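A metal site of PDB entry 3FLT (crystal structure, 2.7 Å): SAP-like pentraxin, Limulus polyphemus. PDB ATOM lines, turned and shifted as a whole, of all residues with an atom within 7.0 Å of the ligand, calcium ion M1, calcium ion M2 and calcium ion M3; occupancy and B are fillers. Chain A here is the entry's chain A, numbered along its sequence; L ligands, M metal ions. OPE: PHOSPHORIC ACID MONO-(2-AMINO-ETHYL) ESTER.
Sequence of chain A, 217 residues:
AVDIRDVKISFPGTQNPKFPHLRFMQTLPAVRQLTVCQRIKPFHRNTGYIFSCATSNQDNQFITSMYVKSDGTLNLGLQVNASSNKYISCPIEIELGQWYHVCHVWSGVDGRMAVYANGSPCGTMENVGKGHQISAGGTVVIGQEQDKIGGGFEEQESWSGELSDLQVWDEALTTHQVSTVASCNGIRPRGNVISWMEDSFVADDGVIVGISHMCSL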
ATOM      1  N   THR A  47      11.920  35.580  13.592  1.00  0.00           N
ATOM      2  CA  THR A  47      11.281  34.937  14.729  1.00  0.00           C
ATOM      3  C   THR A  47      12.043  33.769  15.298  1.00  0.00           C
ATOM      4  O   THR A  47      12.547  32.912  14.564  1.00  0.00           O
ATOM      5  CB  THR A  47       9.865  34.444  14.344  1.00  0.00           C
ATOM      6  OG1 THR A  47       9.018  35.576  14.098  1.00  0.00           O
ATOM      7  CG2 THR A  47       9.243  33.610  15.451  1.00  0.00           C
ATOM      8  N   TYR A  49      12.042  31.158  19.051  1.00  0.00           N
ATOM      9  CA  TYR A  49      11.409  30.822  20.321  1.00  0.00           C
ATOM     10  C   TYR A  49      12.471  30.708  21.392  1.00  0.00           C
ATOM     11  O   TYR A  49      13.454  29.973  21.230  1.00  0.00           O
ATOM     12  CB  TYR A  49      10.606  29.520  20.208  1.00  0.00           C
ATOM     13  CG  TYR A  49       9.404  29.670  19.318  1.00  0.00           C
ATOM     14  CD1 TYR A  49       9.466  29.331  17.957  1.00  0.00           C
ATOM     15  CD2 TYR A  49       8.223  30.234  19.795  1.00  0.00           C
ATOM     16  CE1 TYR A  49       8.385  29.562  17.108  1.00  0.00           C
ATOM     17  CE2 TYR A  49       7.148  30.468  18.962  1.00  0.00           C
ATOM     18  CZ  TYR A  49       7.234  30.127  17.616  1.00  0.00           C
ATOM     19  OH  TYR A  49       6.178  30.396  16.796  1.00  0.00           O
ATOM     20  N   SER A  52      10.334  27.556  25.891  1.00  0.00           N
ATOM     21  CA  SER A  52       9.351  26.583  25.408  1.00  0.00           C
ATOM     22  C   SER A  52       8.970  25.596  26.506  1.00  0.00           C
ATOM     23  O   SER A  52       9.839  24.946  27.100  1.00  0.00           O
ATOM     24  CB  SER A  52       9.927  25.813  24.219  1.00  0.00           C
ATOM     25  OG  SER A  52       9.174  24.651  23.925  1.00  0.00           O
ATOM     26  N   ALA A  54       6.438  22.286  27.399  1.00  0.00           N
ATOM     27  CA  ALA A  54       5.578  21.250  26.854  1.00  0.00           C
ATOM     28  C   ALA A  54       5.272  20.114  27.811  1.00  0.00           C
ATOM     29  O   ALA A  54       6.072  19.758  28.665  1.00  0.00           O
ATOM     30  CB  ALA A  54       6.206  20.683  25.589  1.00  0.00           C
ATOM     31  N   GLN A  58       0.259  18.329  25.444  1.00  0.00           N
ATOM     32  CA  GLN A  58       0.337  19.620  24.761  1.00  0.00           C
ATOM     33  C   GLN A  58       1.775  20.120  24.682  1.00  0.00           C
ATOM     34  O   GLN A  58       2.347  20.523  25.682  1.00  0.00           O
ATOM     35  CB  GLN A  58      -0.524  20.645  25.513  1.00  0.00           C
ATOM     36  CG  GLN A  58      -0.427  22.075  25.008  1.00  0.00           C
ATOM     37  CD  GLN A  58      -0.900  22.230  23.566  1.00  0.00           C
ATOM     38  OE1 GLN A  58      -0.177  21.874  22.628  1.00  0.00           O
ATOM     39  NE2 GLN A  58      -2.114  22.753  23.388  1.00  0.00           N
ATOM     40  N   ASP A  59       2.345  20.099  23.477  1.00  0.00           N
ATOM     41  CA  ASP A  59       3.723  20.543  23.279  1.00  0.00           C
ATOM     42  C   ASP A  59       3.835  22.078  23.241  1.00  0.00           C
ATOM     43  O   ASP A  59       4.930  22.629  23.357  1.00  0.00           O
ATOM     44  CB  ASP A  59       4.278  19.932  21.981  1.00  0.00           C
ATOM     45  CG  ASP A  59       3.469  20.308  20.750  1.00  0.00           C
ATOM     46  OD1 ASP A  59       2.253  20.012  20.713  1.00  0.00           O
ATOM     47  OD2 ASP A  59       4.046  20.921  19.825  1.00  0.00           O
ATOM     48  N   ASN A  60       2.703  22.760  23.093  1.00  0.00           N
ATOM     49  CA  ASN A  60       2.694  24.207  23.065  1.00  0.00           C
ATOM     50  C   ASN A  60       1.947  24.777  24.266  1.00  0.00           C
ATOM     51  O   ASN A  60       0.994  25.542  24.109  1.00  0.00           O
ATOM     52  CB  ASN A  60       2.032  24.723  21.776  1.00  0.00           C
ATOM     53  CG  ASN A  60       2.850  24.418  20.529  1.00  0.00           C
ATOM     54  OD1 ASN A  60       3.728  23.559  20.544  1.00  0.00           O
ATOM     55  ND2 ASN A  60       2.557  25.124  19.442  1.00  0.00           N
ATOM     56  N   ILE A  63       4.963  29.299  25.164  1.00  0.00           N
ATOM     57  CA  ILE A  63       6.133  29.577  24.335  1.00  0.00           C
ATOM     58  C   ILE A  63       6.342  31.066  24.103  1.00  0.00           C
ATOM     59  O   ILE A  63       5.457  31.742  23.601  1.00  0.00           O
ATOM     60  CB  ILE A  63       6.012  28.948  22.931  1.00  0.00           C
ATOM     61  CG1 ILE A  63       4.920  27.871  22.934  1.00  0.00           C
ATOM     62  CG2 ILE A  63       7.358  28.380  22.511  1.00  0.00           C
ATOM     63  CD1 ILE A  63       4.628  27.303  21.539  1.00  0.00           C
ATOM     64  N   GLN A  79       2.521  32.415  23.229  1.00  0.00           N
ATOM     65  CA  GLN A  79       1.552  31.445  22.779  1.00  0.00           C
ATOM     66  C   GLN A  79       1.192  30.557  23.958  1.00  0.00           C
ATOM     67  O   GLN A  79       2.077  30.018  24.614  1.00  0.00           O
ATOM     68  CB  GLN A  79       2.115  30.597  21.628  1.00  0.00           C
ATOM     69  CG  GLN A  79       1.157  29.498  21.162  1.00  0.00           C
ATOM     70  CD  GLN A  79       1.711  28.659  20.015  1.00  0.00           C
ATOM     71  OE1 GLN A  79       1.240  27.557  19.760  1.00  0.00           O
ATOM     72  NE2 GLN A  79       2.719  29.186  19.315  1.00  0.00           N
ATOM     73  N   SER A  83      -2.400  28.400  21.124  1.00  0.00           N
ATOM     74  CA  SER A  83      -3.139  29.478  20.486  1.00  0.00           C
ATOM     75  C   SER A  83      -2.207  30.008  19.408  1.00  0.00           C
ATOM     76  O   SER A  83      -1.142  29.443  19.175  1.00  0.00           O
ATOM     77  CB  SER A  83      -3.459  30.594  21.492  1.00  0.00           C
ATOM     78  OG  SER A  83      -2.275  31.260  21.924  1.00  0.00           O
ATOM     79  N   ASN A  85       0.448  32.793  17.954  1.00  0.00           N
ATOM     80  CA  ASN A  85       1.395  33.669  18.625  1.00  0.00           C
ATOM     81  C   ASN A  85       0.842  35.081  18.678  1.00  0.00           C
ATOM     82  O   ASN A  85       0.505  35.659  17.649  1.00  0.00           O
ATOM     83  CB  ASN A  85       2.740  33.661  17.918  1.00  0.00           C
ATOM     84  CG  ASN A  85       3.459  32.353  18.074  1.00  0.00           C
ATOM     85  OD1 ASN A  85       3.705  31.901  19.191  1.00  0.00           O
ATOM     86  ND2 ASN A  85       3.801  31.732  16.961  1.00  0.00           N
ATOM     87  N   GLU A 145      12.136  25.202  19.919  1.00  0.00           N
ATOM     88  CA  GLU A 145      10.690  25.027  20.129  1.00  0.00           C
ATOM     89  C   GLU A 145      10.331  23.540  20.070  1.00  0.00           C
ATOM     90  O   GLU A 145      10.476  22.888  19.036  1.00  0.00           O
ATOM     91  CB  GLU A 145       9.916  25.797  19.048  1.00  0.00           C
ATOM     92  CG  GLU A 145       8.492  26.170  19.402  1.00  0.00           C
ATOM     93  CD  GLU A 145       7.548  24.967  19.463  1.00  0.00           C
ATOM     94  OE1 GLU A 145       7.493  24.212  18.468  1.00  0.00           O
ATOM     95  OE2 GLU A 145       6.860  24.788  20.495  1.00  0.00           O
ATOM     96  N   GLN A 146       9.851  23.005  21.191  1.00  0.00           N
ATOM     97  CA  GLN A 146       9.504  21.586  21.278  1.00  0.00           C
ATOM     98  C   GLN A 146       8.231  21.195  20.551  1.00  0.00           C
ATOM     99  O   GLN A 146       7.220  21.884  20.636  1.00  0.00           O
ATOM    100  CB  GLN A 146       9.332  21.176  22.741  1.00  0.00           C
ATOM    101  CG  GLN A 146      10.500  21.443  23.645  1.00  0.00           C
ATOM    102  CD  GLN A 146      10.143  21.209  25.097  1.00  0.00           C
ATOM    103  OE1 GLN A 146      10.122  20.074  25.575  1.00  0.00           O
ATOM    104  NE2 GLN A 146       9.841  22.282  25.811  1.00  0.00           N
ATOM    105  N   ASP A 147       8.283  20.067  19.854  1.00  0.00           N
ATOM    106  CA  ASP A 147       7.102  19.524  19.181  1.00  0.00           C
ATOM    107  C   ASP A 147       6.893  18.190  19.867  1.00  0.00           C
ATOM    108  O   ASP A 147       6.000  17.426  19.538  1.00  0.00           O
ATOM    109  CB  ASP A 147       7.338  19.321  17.695  1.00  0.00           C
ATOM    110  CG  ASP A 147       7.307  20.614  16.919  1.00  0.00           C
ATOM    111  OD1 ASP A 147       6.426  21.438  17.192  1.00  0.00           O
ATOM    112  OD2 ASP A 147       8.155  20.807  16.033  1.00  0.00           O
ATOM    113  N   LYS A 148       7.746  17.942  20.845  1.00  0.00           N
ATOM    114  CA  LYS A 148       7.749  16.721  21.632  1.00  0.00           C
ATOM    115  C   LYS A 148       8.562  17.015  22.901  1.00  0.00           C
ATOM    116  O   LYS A 148       9.455  17.869  22.887  1.00  0.00           O
ATOM    117  CB  LYS A 148       8.410  15.612  20.828  1.00  0.00           C
ATOM    118  CG  LYS A 148       8.642  14.363  21.597  1.00  0.00           C
ATOM    119  CD  LYS A 148       9.292  13.329  20.714  1.00  0.00           C
ATOM    120  CE  LYS A 148      10.627  13.790  20.205  1.00  0.00           C
ATOM    121  NZ  LYS A 148      11.338  12.667  19.533  1.00  0.00           N
ATOM    122  N   GLY A 151      12.236  17.683  22.579  1.00  0.00           N
ATOM    123  CA  GLY A 151      12.692  17.479  21.221  1.00  0.00           C
ATOM    124  C   GLY A 151      11.758  17.919  20.098  1.00  0.00           C
ATOM    125  O   GLY A 151      10.862  18.741  20.302  1.00  0.00           O
ATOM    126  N   GLY A 152      11.990  17.356  18.911  1.00  0.00           N
ATOM    127  CA  GLY A 152      11.192  17.707  17.754  1.00  0.00           C
ATOM    128  C   GLY A 152      11.441  19.149  17.379  1.00  0.00           C
ATOM    129  O   GLY A 152      10.502  19.884  17.069  1.00  0.00           O
ATOM    130  N   PHE A 153      12.702  19.563  17.384  1.00  0.00           N
ATOM    131  CA  PHE A 153      13.047  20.940  17.065  1.00  0.00           C
ATOM    132  C   PHE A 153      13.057  21.248  15.567  1.00  0.00           C
ATOM    133  O   PHE A 153      13.363  20.376  14.760  1.00  0.00           O
ATOM    134  CB  PHE A 153      14.414  21.297  17.654  1.00  0.00           C
ATOM    135  CG  PHE A 153      14.555  20.957  19.123  1.00  0.00           C
ATOM    136  CD1 PHE A 153      13.572  21.341  20.047  1.00  0.00           C
ATOM    137  CD2 PHE A 153      15.684  20.274  19.587  1.00  0.00           C
ATOM    138  CE1 PHE A 153      13.727  21.060  21.410  1.00  0.00           C
ATOM    139  CE2 PHE A 153      15.839  19.993  20.950  1.00  0.00           C
ATOM    140  CZ  PHE A 153      14.856  20.382  21.860  1.00  0.00           C
ATOM    141  N   GLU A 154      12.712  22.480  15.231  1.00  0.00           N
ATOM    142  CA  GLU A 154      12.693  22.960  13.846  1.00  0.00           C
ATOM    143  C   GLU A 154      13.677  24.128  13.760  1.00  0.00           C
ATOM    144  O   GLU A 154      13.609  25.047  14.569  1.00  0.00           O
ATOM    145  CB  GLU A 154      11.286  23.422  13.467  1.00  0.00           C
ATOM    146  CG  GLU A 154      10.203  22.433  13.840  1.00  0.00           C
ATOM    147  CD  GLU A 154       8.915  22.647  13.060  1.00  0.00           C
ATOM    148  OE1 GLU A 154       8.971  22.577  11.811  1.00  0.00           O
ATOM    149  OE2 GLU A 154       7.858  22.900  13.670  1.00  0.00           O
ATOM    150  N   GLN A 156      13.981  26.708  11.684  1.00  0.00           N
ATOM    151  CA  GLN A 156      13.422  28.036  11.465  1.00  0.00           C
ATOM    152  C   GLN A 156      12.675  28.575  12.663  1.00  0.00           C
ATOM    153  O   GLN A 156      12.178  29.699  12.628  1.00  0.00           O
ATOM    154  CB  GLN A 156      12.547  28.083  10.203  1.00  0.00           C
ATOM    155  CG  GLN A 156      11.109  27.578  10.294  1.00  0.00           C
ATOM    156  CD  GLN A 156      10.986  26.097  10.614  1.00  0.00           C
ATOM    157  OE1 GLN A 156      11.871  25.301  10.299  1.00  0.00           O
ATOM    158  NE2 GLN A 156       9.875  25.728  11.240  1.00  0.00           N
ATOM    159  N   GLU A 157      12.602  27.769  13.731  1.00  0.00           N
ATOM    160  CA  GLU A 157      11.918  28.199  14.952  1.00  0.00           C
ATOM    161  C   GLU A 157      12.879  28.354  16.124  1.00  0.00           C
ATOM    162  O   GLU A 157      12.475  28.693  17.232  1.00  0.00           O
ATOM    163  CB  GLU A 157      10.816  27.199  15.328  1.00  0.00           C
ATOM    164  CG  GLU A 157       9.824  26.930  14.219  1.00  0.00           C
ATOM    165  CD  GLU A 157       8.584  26.197  14.686  1.00  0.00           C
ATOM    166  OE1 GLU A 157       8.694  25.114  15.293  1.00  0.00           O
ATOM    167  OE2 GLU A 157       7.467  26.714  14.450  1.00  0.00           O
HETATM  168  CA  OPE L   1       4.614  26.200  16.563  1.00  0.00           C
HETATM  169  CB  OPE L   1       4.104  27.652  16.436  1.00  0.00           C
HETATM  170  O1  OPE L   1       5.836  23.756  15.456  1.00  0.00           O
HETATM  171  O2  OPE L   1       4.372  23.502  17.494  1.00  0.00           O
HETATM  172  O3  OPE L   1       3.426  22.721  15.308  1.00  0.00           O
HETATM  173  O4  OPE L   1       3.742  25.289  15.852  1.00  0.00           O
HETATM  174  N   OPE L   1       5.041  28.431  15.568  1.00  0.00           N
HETATM  175  P   OPE L   1       4.344  23.813  16.056  1.00  0.00           P
HETATM  176 CA    CA M   1       5.726  22.815  19.430  1.00  0.00          CA
HETATM  177 CA    CA M   2       7.893  23.267  16.352  1.00  0.00          CA
HETATM  178 CA    CA M   3       6.152  24.295  12.962  1.00  0.00          CA
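OH of Tyr 49 is in hydrogen-bond range of N of the ligand (2.6 Å).
The backbone NH (N) of Ile 63 sits at hydrogen-bond distance from the backbone carbonyl oxygen (O) of Gln 79 (3.0 Å).
The side-chain amide nitrogen (ND2) of Asn 85 is in hydrogen-bond range of the side-chain hydroxyl (OH) of Tyr 49.
The side-chain amide nitrogen of Gln 146 sits at hydrogen-bond distance from the backbone carbonyl oxygen of Ser 52 (3.0 Å).
ND2 of Asn 60 lies within hydrogen-bond range of OE1 of Gln 79 (2.8 Å).
The side-chain carboxylate (OE1) of Glu 154 is in hydrogen-bond range of the side-chain amide nitrogen (NE2) of Gln 156, 3.3 Å away.
The side-chain carboxylate (OD2) of Asp 147 lies close to the backbone carbonyl oxygen (O) of Gly 152.
OE1 of Gln 79 lies close to O of Ser 83 (3.1 Å).
N of Tyr 49 is in hydrogen-bond range of O of Glu 157 (3.1 Å).
The nearest printed residue that does not touch calcium ion M1 is Ile 63 (5.1 Å).
NE2 of Gln 79 touches CB of the ligand, at 3.5 Å.
ND2 of Asn 85 touches N of the ligand, at 3.8 Å.
The nearest printed residue that does not touch the ligand is Gln 146 (4.5 Å).
Within 4 Å of calcium ion M2: Glu 145, Asp 147, Glu 154 and Glu 157.
Calcium ion M2 is bound by the side-chain carboxylate (OE1) of Glu 157 (2.3 Å), an oxygen (O1) of the ligand (2.3 Å), the side-chain carboxylate (OE1) of Glu 145 (2.4 Å), the side-chain carboxylate (OD1) of Asp 147 (2.5 Å), the side-chain carboxylate (OD2) of Asp 147 (2.5 Å) and the side-chain carboxylate (OE2) of Glu 154 (2.7 Å).
Calcium ion M2 has six donor atoms within binding distance.
The backbone carbonyl oxygen (O) of Gln 146 is bound to calcium ion M1.
OD1 of Asn 60 binds calcium ion M1.
The side-chain carboxylate (OE1) of Glu 145 is bound to calcium ion M1 (2.4 Å).
Calcium ion M1 is bound by O2 of the ligand (2.5 Å).
OE2 of Glu 145 is bound to calcium ion M1, at 2.5 Å.
OD2 of Asp 59 binds calcium ion M1 (2.6 Å).
OD1 of Asp 147 binds calcium ion M1.
Calcium ion M1 has seven donor atoms within binding distance.
Calcium ion M3 is bound by the side-chain carboxylate (OE2) of Glu 154 (2.3 Å) and an oxygen (O1) of the ligand (2.6 Å).
Calcium ion M3 has two donor atoms within binding distance.
Slightly farther from calcium ion M3 lies the side-chain carboxylate (OE2) of Glu 157 (3.1 Å).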
